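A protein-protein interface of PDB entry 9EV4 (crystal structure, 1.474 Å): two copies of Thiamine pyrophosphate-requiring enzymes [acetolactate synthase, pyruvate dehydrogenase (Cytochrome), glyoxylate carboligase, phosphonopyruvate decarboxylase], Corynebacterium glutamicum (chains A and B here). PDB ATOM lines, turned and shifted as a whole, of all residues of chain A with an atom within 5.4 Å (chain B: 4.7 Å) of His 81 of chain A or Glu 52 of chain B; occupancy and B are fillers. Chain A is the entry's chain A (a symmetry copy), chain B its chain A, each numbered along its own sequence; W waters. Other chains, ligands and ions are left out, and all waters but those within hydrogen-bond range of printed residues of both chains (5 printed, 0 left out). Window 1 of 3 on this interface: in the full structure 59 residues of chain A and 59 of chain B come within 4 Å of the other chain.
OE1 of Glu 52 of chain B lies within hydrogen-bond range of NE2 of His 81 of chain A (3.0 Å).
OE1 of Glu 52 of chain A sits at hydrogen-bond distance from NE2 of His 81 of chain B, 3.0 Å away.
A ring nitrogen (ND1) of His 81 of chain B lies close to the side-chain amide nitrogen (NE2) of Gln 84 of chain A, at 3.4 Å.
The side-chain amide nitrogen (NE2) of Gln 84 of chain B sits at hydrogen-bond distance from the backbone carbonyl oxygen (O) of Pro 77 of chain A.
The side-chain amide nitrogen of Gln 84 of chain B lies close to a ring nitrogen (ND1) of His 81 of chain A (3.4 Å).
A ring nitrogen (ND1) of His 81 of chain B sits at hydrogen-bond distance from the side-chain carboxylate (OE1) of Glu 51 of chain B (2.7 Å).
ND1 of His 81 of chain A sits at hydrogen-bond distance from OE1 of Glu 51 of chain A, 2.7 Å away.
Among the printed residues, merely in contact across the chains: Pro 77 of chain A with Thr 412 of chain B (3.2 Å) and Thr 80 of chain A with Gln 84 of chain B (3.5 Å).
Printed residues of chain B within 4 Å of Thr 80 of chain A: Gln 84.
His 81 of chain A touches two residues of chain B.
Glu 52 of chain B touches just one residue of chain A: His 81 (3.0 Å).
Ala 54 of chain B touches none of the printed residues of chain A.
Ala 55 of chain B touches none of the printed residues of chain A.
Of the printed residues of chain A, His 81 of chain B touches Glu 52 (3.0 Å) and Gln 84 (3.2 Å).
Of the printed residues of chain A, Gln 84 of chain B touches Pro 77 (2.9 Å), Thr 80 (3.5 Å) and His 81 (3.2 Å).
Of the printed residues of chain A, Thr 412 of chain B touches Pro 77.
The nearest residue of chain B that does not touch His 81 of chain A is Thr 412 of chain B (4.3 Å).
Of the 11 printed residues of chain B, 4 touch a printed residue of chain A.
Printed residues of chain B that touch a printed residue of chain A: Glu 52, His 81, Gln 84 and Thr 412.
Among the printed residues, 7 pairs touch across the chains.
Among the printed residues, no Asp or Glu carboxylate lies within 4 Å of a Lys or Arg side-chain nitrogen of the other chain.
Glu 52 of chain A touches His 81 of chain B, and with the chains exchanged His 81 of chain A touches Glu 52 of chain B.
His 81 of chain A touches Gln 84 of chain B, and with the chains exchanged Gln 84 of chain A touches His 81 of chain B.
Water W5 lies within hydrogen-bond range of OG1 of Thr 412 of chain B (2.7 Å), OE2 of Glu 52 of chain B (2.7 Å) and NE2 of His 81 of chain A (3.5 Å).
Water W3 lies within hydrogen-bond range of the side-chain carboxylate (OE2) of Glu 52 of chain A (2.7 Å) and a ring nitrogen (NE2) of His 81 of chain B (3.5 Å).
Water W1 bridges OE1 of Glu 52 of chain A (2.8 Å) and NE2 of His 81 of chain B (3.4 Å).
Water W2 lies within hydrogen-bond range of the side-chain carboxylate of Glu 52 of chain B (2.8 Å), a ring nitrogen (NE2) of His 81 of chain A (3.4 Å) and the side-chain sulfur of Met 443 of chain B (3.5 Å).
Water W4 lies within hydrogen-bond range of the side-chain carboxylate of Glu 51 of chain A (2.8 Å) and the side-chain hydroxyl of Thr 412 of chain B (3.1 Å).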
ATOM      1  N   GLU A  51      31.531  17.350   8.095  1.00  0.00           N
ATOM      2  CA  GLU A  51      30.141  17.452   7.654  1.00  0.00           C
ATOM      3  C   GLU A  51      29.838  18.818   7.013  1.00  0.00           C
ATOM      4  O   GLU A  51      29.023  18.901   6.091  1.00  0.00           O
ATOM      5  CB  GLU A  51      29.171  17.261   8.852  1.00  0.00           C
ATOM      6  CG  GLU A  51      29.346  16.001   9.677  1.00  0.00           C
ATOM      7  CD  GLU A  51      28.330  15.829  10.799  1.00  0.00           C
ATOM      8  OE1 GLU A  51      28.431  16.562  11.809  1.00  0.00           O
ATOM      9  OE2 GLU A  51      27.461  14.936  10.684  1.00  0.00           O
ATOM     10  N   GLU A  52      30.536  19.894   7.503  1.00  0.00           N
ATOM     11  CA  GLU A  52      30.291  21.250   6.946  1.00  0.00           C
ATOM     12  C   GLU A  52      30.643  21.334   5.451  1.00  0.00           C
ATOM     13  O   GLU A  52      30.139  22.214   4.742  1.00  0.00           O
ATOM     14  CB  GLU A  52      31.107  22.316   7.713  1.00  0.00           C
ATOM     15  CG  GLU A  52      30.946  23.715   7.124  1.00  0.00           C
ATOM     16  CD  GLU A  52      31.605  24.843   7.901  1.00  0.00           C
ATOM     17  OE1 GLU A  52      31.590  24.765   9.154  1.00  0.00           O
ATOM     18  OE2 GLU A  52      32.122  25.799   7.262  1.00  0.00           O
ATOM     19  N   PRO A  77      22.686  17.514  15.273  1.00  0.00           N
ATOM     20  CA  PRO A  77      23.954  18.225  14.947  1.00  0.00           C
ATOM     21  C   PRO A  77      24.405  18.071  13.495  1.00  0.00           C
ATOM     22  O   PRO A  77      24.985  18.998  12.917  1.00  0.00           O
ATOM     23  CB  PRO A  77      25.013  17.563  15.860  1.00  0.00           C
ATOM     24  CG  PRO A  77      24.301  16.719  16.798  1.00  0.00           C
ATOM     25  CD  PRO A  77      22.816  16.601  16.422  1.00  0.00           C
ATOM     26  N   GLY A  78      24.149  16.911  12.900  1.00  0.00           N
ATOM     27  CA  GLY A  78      24.508  16.682  11.494  1.00  0.00           C
ATOM     28  C   GLY A  78      23.932  17.745  10.542  1.00  0.00           C
ATOM     29  O   GLY A  78      24.672  18.378   9.774  1.00  0.00           O
ATOM     30  N   ASN A  79      22.595  17.974  10.593  1.00  0.00           N
ATOM     31  CA  ASN A  79      22.058  18.877   9.585  1.00  0.00           C
ATOM     32  C   ASN A  79      22.346  20.346  10.033  1.00  0.00           C
ATOM     33  O   ASN A  79      22.407  21.173   9.141  1.00  0.00           O
ATOM     34  CB  ASN A  79      20.620  18.544   9.157  1.00  0.00           C
ATOM     35  CG  ASN A  79      19.595  18.898  10.161  1.00  0.00           C
ATOM     36  OD1 ASN A  79      19.781  19.834  10.910  1.00  0.00           O
ATOM     37  ND2 ASN A  79      18.490  18.178  10.170  1.00  0.00           N
ATOM     38  N   THR A  80      22.673  20.641  11.319  1.00  0.00           N
ATOM     39  CA  THR A  80      23.128  21.943  11.725  1.00  0.00           C
ATOM     40  C   THR A  80      24.419  22.319  10.945  1.00  0.00           C
ATOM     41  O   THR A  80      24.604  23.479  10.540  1.00  0.00           O
ATOM     42  CB  THR A  80      23.303  21.940  13.254  1.00  0.00           C
ATOM     43  OG1 THR A  80      22.013  21.648  13.819  1.00  0.00           O
ATOM     44  CG2 THR A  80      23.810  23.248  13.758  1.00  0.00           C
ATOM     45  N   HIS A  81      25.271  21.311  10.638  1.00  0.00           N
ATOM     46  CA  HIS A  81      26.488  21.566   9.861  1.00  0.00           C
ATOM     47  C   HIS A  81      26.198  21.895   8.376  1.00  0.00           C
ATOM     48  O   HIS A  81      27.125  22.337   7.683  1.00  0.00           O
ATOM     49  CB  HIS A  81      27.420  20.350   9.951  1.00  0.00           C
ATOM     50  CG  HIS A  81      28.288  20.394  11.181  1.00  0.00           C
ATOM     51  ND1 HIS A  81      28.467  19.273  11.983  1.00  0.00           N
ATOM     52  CD2 HIS A  81      29.003  21.414  11.695  1.00  0.00           C
ATOM     53  CE1 HIS A  81      29.284  19.648  12.956  1.00  0.00           C
ATOM     54  NE2 HIS A  81      29.653  20.924  12.822  1.00  0.00           N
ATOM     55  N   LEU A  82      24.957  21.683   7.875  1.00  0.00           N
ATOM     56  CA  LEU A  82      24.653  22.075   6.481  1.00  0.00           C
ATOM     57  C   LEU A  82      24.521  23.594   6.318  1.00  0.00           C
ATOM     58  O   LEU A  82      24.554  24.081   5.207  1.00  0.00           O
ATOM     59  CB  LEU A  82      23.297  21.479   6.006  1.00  0.00           C
ATOM     60  CG  LEU A  82      23.246  19.931   5.890  1.00  0.00           C
ATOM     61  CD1 LEU A  82      21.755  19.426   5.733  1.00  0.00           C
ATOM     62  CD2 LEU A  82      24.101  19.442   4.718  1.00  0.00           C
ATOM     63  N   ILE A  83      24.191  24.316   7.400  1.00  0.00           N
ATOM     64  CA  ILE A  83      23.755  25.713   7.292  1.00  0.00           C
ATOM     65  C   ILE A  83      24.731  26.623   6.543  1.00  0.00           C
ATOM     66  O   ILE A  83      24.298  27.326   5.624  1.00  0.00           O
ATOM     67  CB  ILE A  83      23.473  26.289   8.691  1.00  0.00           C
ATOM     68  CG1 ILE A  83      22.331  25.489   9.383  1.00  0.00           C
ATOM     69  CG2 ILE A  83      23.078  27.792   8.612  1.00  0.00           C
ATOM     70  CD1 ILE A  83      22.138  25.884  10.918  1.00  0.00           C
ATOM     71  N   GLN A  84      26.033  26.609   6.903  1.00  0.00           N
ATOM     72  CA  GLN A  84      26.974  27.545   6.260  1.00  0.00           C
ATOM     73  C   GLN A  84      27.014  27.355   4.743  1.00  0.00           C
ATOM     74  O   GLN A  84      26.936  28.350   3.995  1.00  0.00           O
ATOM     75  CB  GLN A  84      28.384  27.390   6.866  1.00  0.00           C
ATOM     76  CG  GLN A  84      29.235  28.631   6.709  1.00  0.00           C
ATOM     77  CD  GLN A  84      28.866  29.669   7.744  1.00  0.00           C
ATOM     78  OE1 GLN A  84      27.959  30.437   7.537  1.00  0.00           O
ATOM     79  NE2 GLN A  84      29.555  29.711   8.901  1.00  0.00           N
ATOM     80  N   GLY A  85      27.138  26.102   4.308  1.00  0.00           N
ATOM     81  CA  GLY A  85      27.254  25.788   2.889  1.00  0.00           C
ATOM     82  C   GLY A  85      25.949  26.026   2.153  1.00  0.00           C
ATOM     83  O   GLY A  85      25.961  26.284   0.952  1.00  0.00           O
ATOM     84  N   ASN B  50      39.375  27.666  15.038  1.00  0.00           N
ATOM     85  CA  ASN B  50      38.126  27.197  14.416  1.00  0.00           C
ATOM     86  C   ASN B  50      37.024  27.969  15.107  1.00  0.00           C
ATOM     87  O   ASN B  50      36.860  27.812  16.325  1.00  0.00           O
ATOM     88  CB  ASN B  50      37.954  25.678  14.593  1.00  0.00           C
ATOM     89  CG  ASN B  50      38.922  24.858  13.763  1.00  0.00           C
ATOM     90  OD1 ASN B  50      39.388  25.306  12.715  1.00  0.00           O
ATOM     91  ND2 ASN B  50      39.193  23.640  14.189  1.00  0.00           N
ATOM     92  N   GLU B  51      36.259  28.823  14.384  1.00  0.00           N
ATOM     93  CA  GLU B  51      35.210  29.619  15.021  1.00  0.00           C
ATOM     94  C   GLU B  51      34.192  28.740  15.767  1.00  0.00           C
ATOM     95  O   GLU B  51      33.656  29.155  16.798  1.00  0.00           O
ATOM     96  CB  GLU B  51      34.437  30.452  13.963  1.00  0.00           C
ATOM     97  CG  GLU B  51      35.264  31.343  13.057  1.00  0.00           C
ATOM     98  CD  GLU B  51      34.455  32.187  12.081  1.00  0.00           C
ATOM     99  OE1 GLU B  51      33.916  31.615  11.107  1.00  0.00           O
ATOM    100  OE2 GLU B  51      34.394  33.422  12.271  1.00  0.00           O
ATOM    101  N   GLU B  52      33.954  27.494  15.241  1.00  0.00           N
ATOM    102  CA  GLU B  52      32.974  26.590  15.896  1.00  0.00           C
ATOM    103  C   GLU B  52      33.394  26.221  17.329  1.00  0.00           C
ATOM    104  O   GLU B  52      32.548  25.838  18.147  1.00  0.00           O
ATOM    105  CB  GLU B  52      32.792  25.290  15.078  1.00  0.00           C
ATOM    106  CG  GLU B  52      31.852  24.296  15.756  1.00  0.00           C
ATOM    107  CD  GLU B  52      31.511  23.052  14.953  1.00  0.00           C
ATOM    108  OE1 GLU B  52      31.374  23.185  13.713  1.00  0.00           O
ATOM    109  OE2 GLU B  52      31.373  21.956  15.561  1.00  0.00           O
ATOM    110  N   ALA B  53      34.697  26.277  17.626  1.00  0.00           N
ATOM    111  CA  ALA B  53      35.165  25.892  18.956  1.00  0.00           C
ATOM    112  C   ALA B  53      34.755  26.874  20.063  1.00  0.00           C
ATOM    113  O   ALA B  53      34.697  26.470  21.221  1.00  0.00           O
ATOM    114  CB  ALA B  53      36.700  25.749  18.944  1.00  0.00           C
ATOM    115  N   ALA B  54      34.557  28.172  19.736  1.00  0.00           N
ATOM    116  CA  ALA B  54      34.383  29.208  20.767  1.00  0.00           C
ATOM    117  C   ALA B  54      33.267  28.908  21.745  1.00  0.00           C
ATOM    118  O   ALA B  54      33.471  29.053  22.962  1.00  0.00           O
ATOM    119  CB  ALA B  54      34.151  30.579  20.119  1.00  0.00           C
ATOM    120  N   ALA B  55      32.118  28.463  21.237  1.00  0.00           N
ATOM    121  CA  ALA B  55      30.944  28.273  22.099  1.00  0.00           C
ATOM    122  C   ALA B  55      31.110  26.995  22.949  1.00  0.00           C
ATOM    123  O   ALA B  55      30.631  26.946  24.098  1.00  0.00           O
ATOM    124  CB  ALA B  55      29.667  28.239  21.257  1.00  0.00           C
ATOM    125  N   PHE B  56      31.819  25.960  22.411  1.00  0.00           N
ATOM    126  CA  PHE B  56      32.100  24.767  23.249  1.00  0.00           C
ATOM    127  C   PHE B  56      33.080  25.131  24.361  1.00  0.00           C
ATOM    128  O   PHE B  56      32.933  24.655  25.495  1.00  0.00           O
ATOM    129  CB  PHE B  56      32.742  23.660  22.406  1.00  0.00           C
ATOM    130  CG  PHE B  56      31.814  23.028  21.416  1.00  0.00           C
ATOM    131  CD1 PHE B  56      30.914  22.044  21.810  1.00  0.00           C
ATOM    132  CD2 PHE B  56      31.824  23.418  20.090  1.00  0.00           C
ATOM    133  CE1 PHE B  56      30.111  21.397  20.871  1.00  0.00           C
ATOM    134  CE2 PHE B  56      30.953  22.822  19.160  1.00  0.00           C
ATOM    135  CZ  PHE B  56      30.130  21.792  19.553  1.00  0.00           C
ATOM    136  N   HIS B  81      28.645  29.970  12.954  1.00  0.00           N
ATOM    137  CA  HIS B  81      29.504  28.951  13.564  1.00  0.00           C
ATOM    138  C   HIS B  81      29.282  28.810  15.090  1.00  0.00           C
ATOM    139  O   HIS B  81      29.791  27.840  15.668  1.00  0.00           O
ATOM    140  CB  HIS B  81      30.975  29.282  13.282  1.00  0.00           C
ATOM    141  CG  HIS B  81      31.426  28.753  11.946  1.00  0.00           C
ATOM    142  ND1 HIS B  81      32.171  29.533  11.070  1.00  0.00           N
ATOM    143  CD2 HIS B  81      31.233  27.540  11.390  1.00  0.00           C
ATOM    144  CE1 HIS B  81      32.406  28.771  10.013  1.00  0.00           C
ATOM    145  NE2 HIS B  81      31.880  27.553  10.159  1.00  0.00           N
ATOM    146  N   GLN B  84      26.325  25.245  16.814  1.00  0.00           N
ATOM    147  CA  GLN B  84      26.519  23.891  17.365  1.00  0.00           C
ATOM    148  C   GLN B  84      26.885  23.932  18.850  1.00  0.00           C
ATOM    149  O   GLN B  84      26.290  23.185  19.652  1.00  0.00           O
ATOM    150  CB  GLN B  84      27.594  23.132  16.560  1.00  0.00           C
ATOM    151  CG  GLN B  84      27.455  21.629  16.660  1.00  0.00           C
ATOM    152  CD  GLN B  84      26.363  21.128  15.742  1.00  0.00           C
ATOM    153  OE1 GLN B  84      25.216  21.117  16.114  1.00  0.00           O
ATOM    154  NE2 GLN B  84      26.691  20.713  14.504  1.00  0.00           N
ATOM    155  N   THR B 412      26.830  16.039  19.484  1.00  0.00           N
ATOM    156  CA  THR B 412      27.573  16.477  18.297  1.00  0.00           C
ATOM    157  C   THR B 412      29.007  15.955  18.345  1.00  0.00           C
ATOM    158  O   THR B 412      29.589  15.800  19.418  1.00  0.00           O
ATOM    159  CB  THR B 412      27.550  18.004  18.171  1.00  0.00           C
ATOM    160  OG1 THR B 412      27.974  18.355  16.844  1.00  0.00           O
ATOM    161  CG2 THR B 412      28.393  18.688  19.236  1.00  0.00           C
ATOM    162  N   MET B 443      38.751  18.365  12.217  1.00  0.00           N
ATOM    163  CA  MET B 443      39.022  19.775  12.586  1.00  0.00           C
ATOM    164  C   MET B 443      40.212  19.893  13.564  1.00  0.00           C
ATOM    165  O   MET B 443      40.414  20.934  14.164  1.00  0.00           O
ATOM    166  CB  MET B 443      37.775  20.426  13.252  1.00  0.00           C
ATOM    167  CG  MET B 443      36.559  20.602  12.286  1.00  0.00           C
ATOM    168  SD  MET B 443      35.275  21.443  13.304  1.00  0.00           S
ATOM    169  CE  MET B 443      35.752  23.127  13.086  1.00  0.00           C
HETATM  170  O   HOH W   1      33.414  24.694  11.302  1.00  0.00           O
HETATM  171  O   HOH W   2      32.489  22.174  11.329  1.00  0.00           O
HETATM  172  O   HOH W   3      32.753  28.428   6.885  1.00  0.00           O
HETATM  173  O   HOH W   4      27.993  16.283  14.591  1.00  0.00           O
HETATM  174  O   HOH W   5      30.205  19.525  15.982  1.00  0.00           O
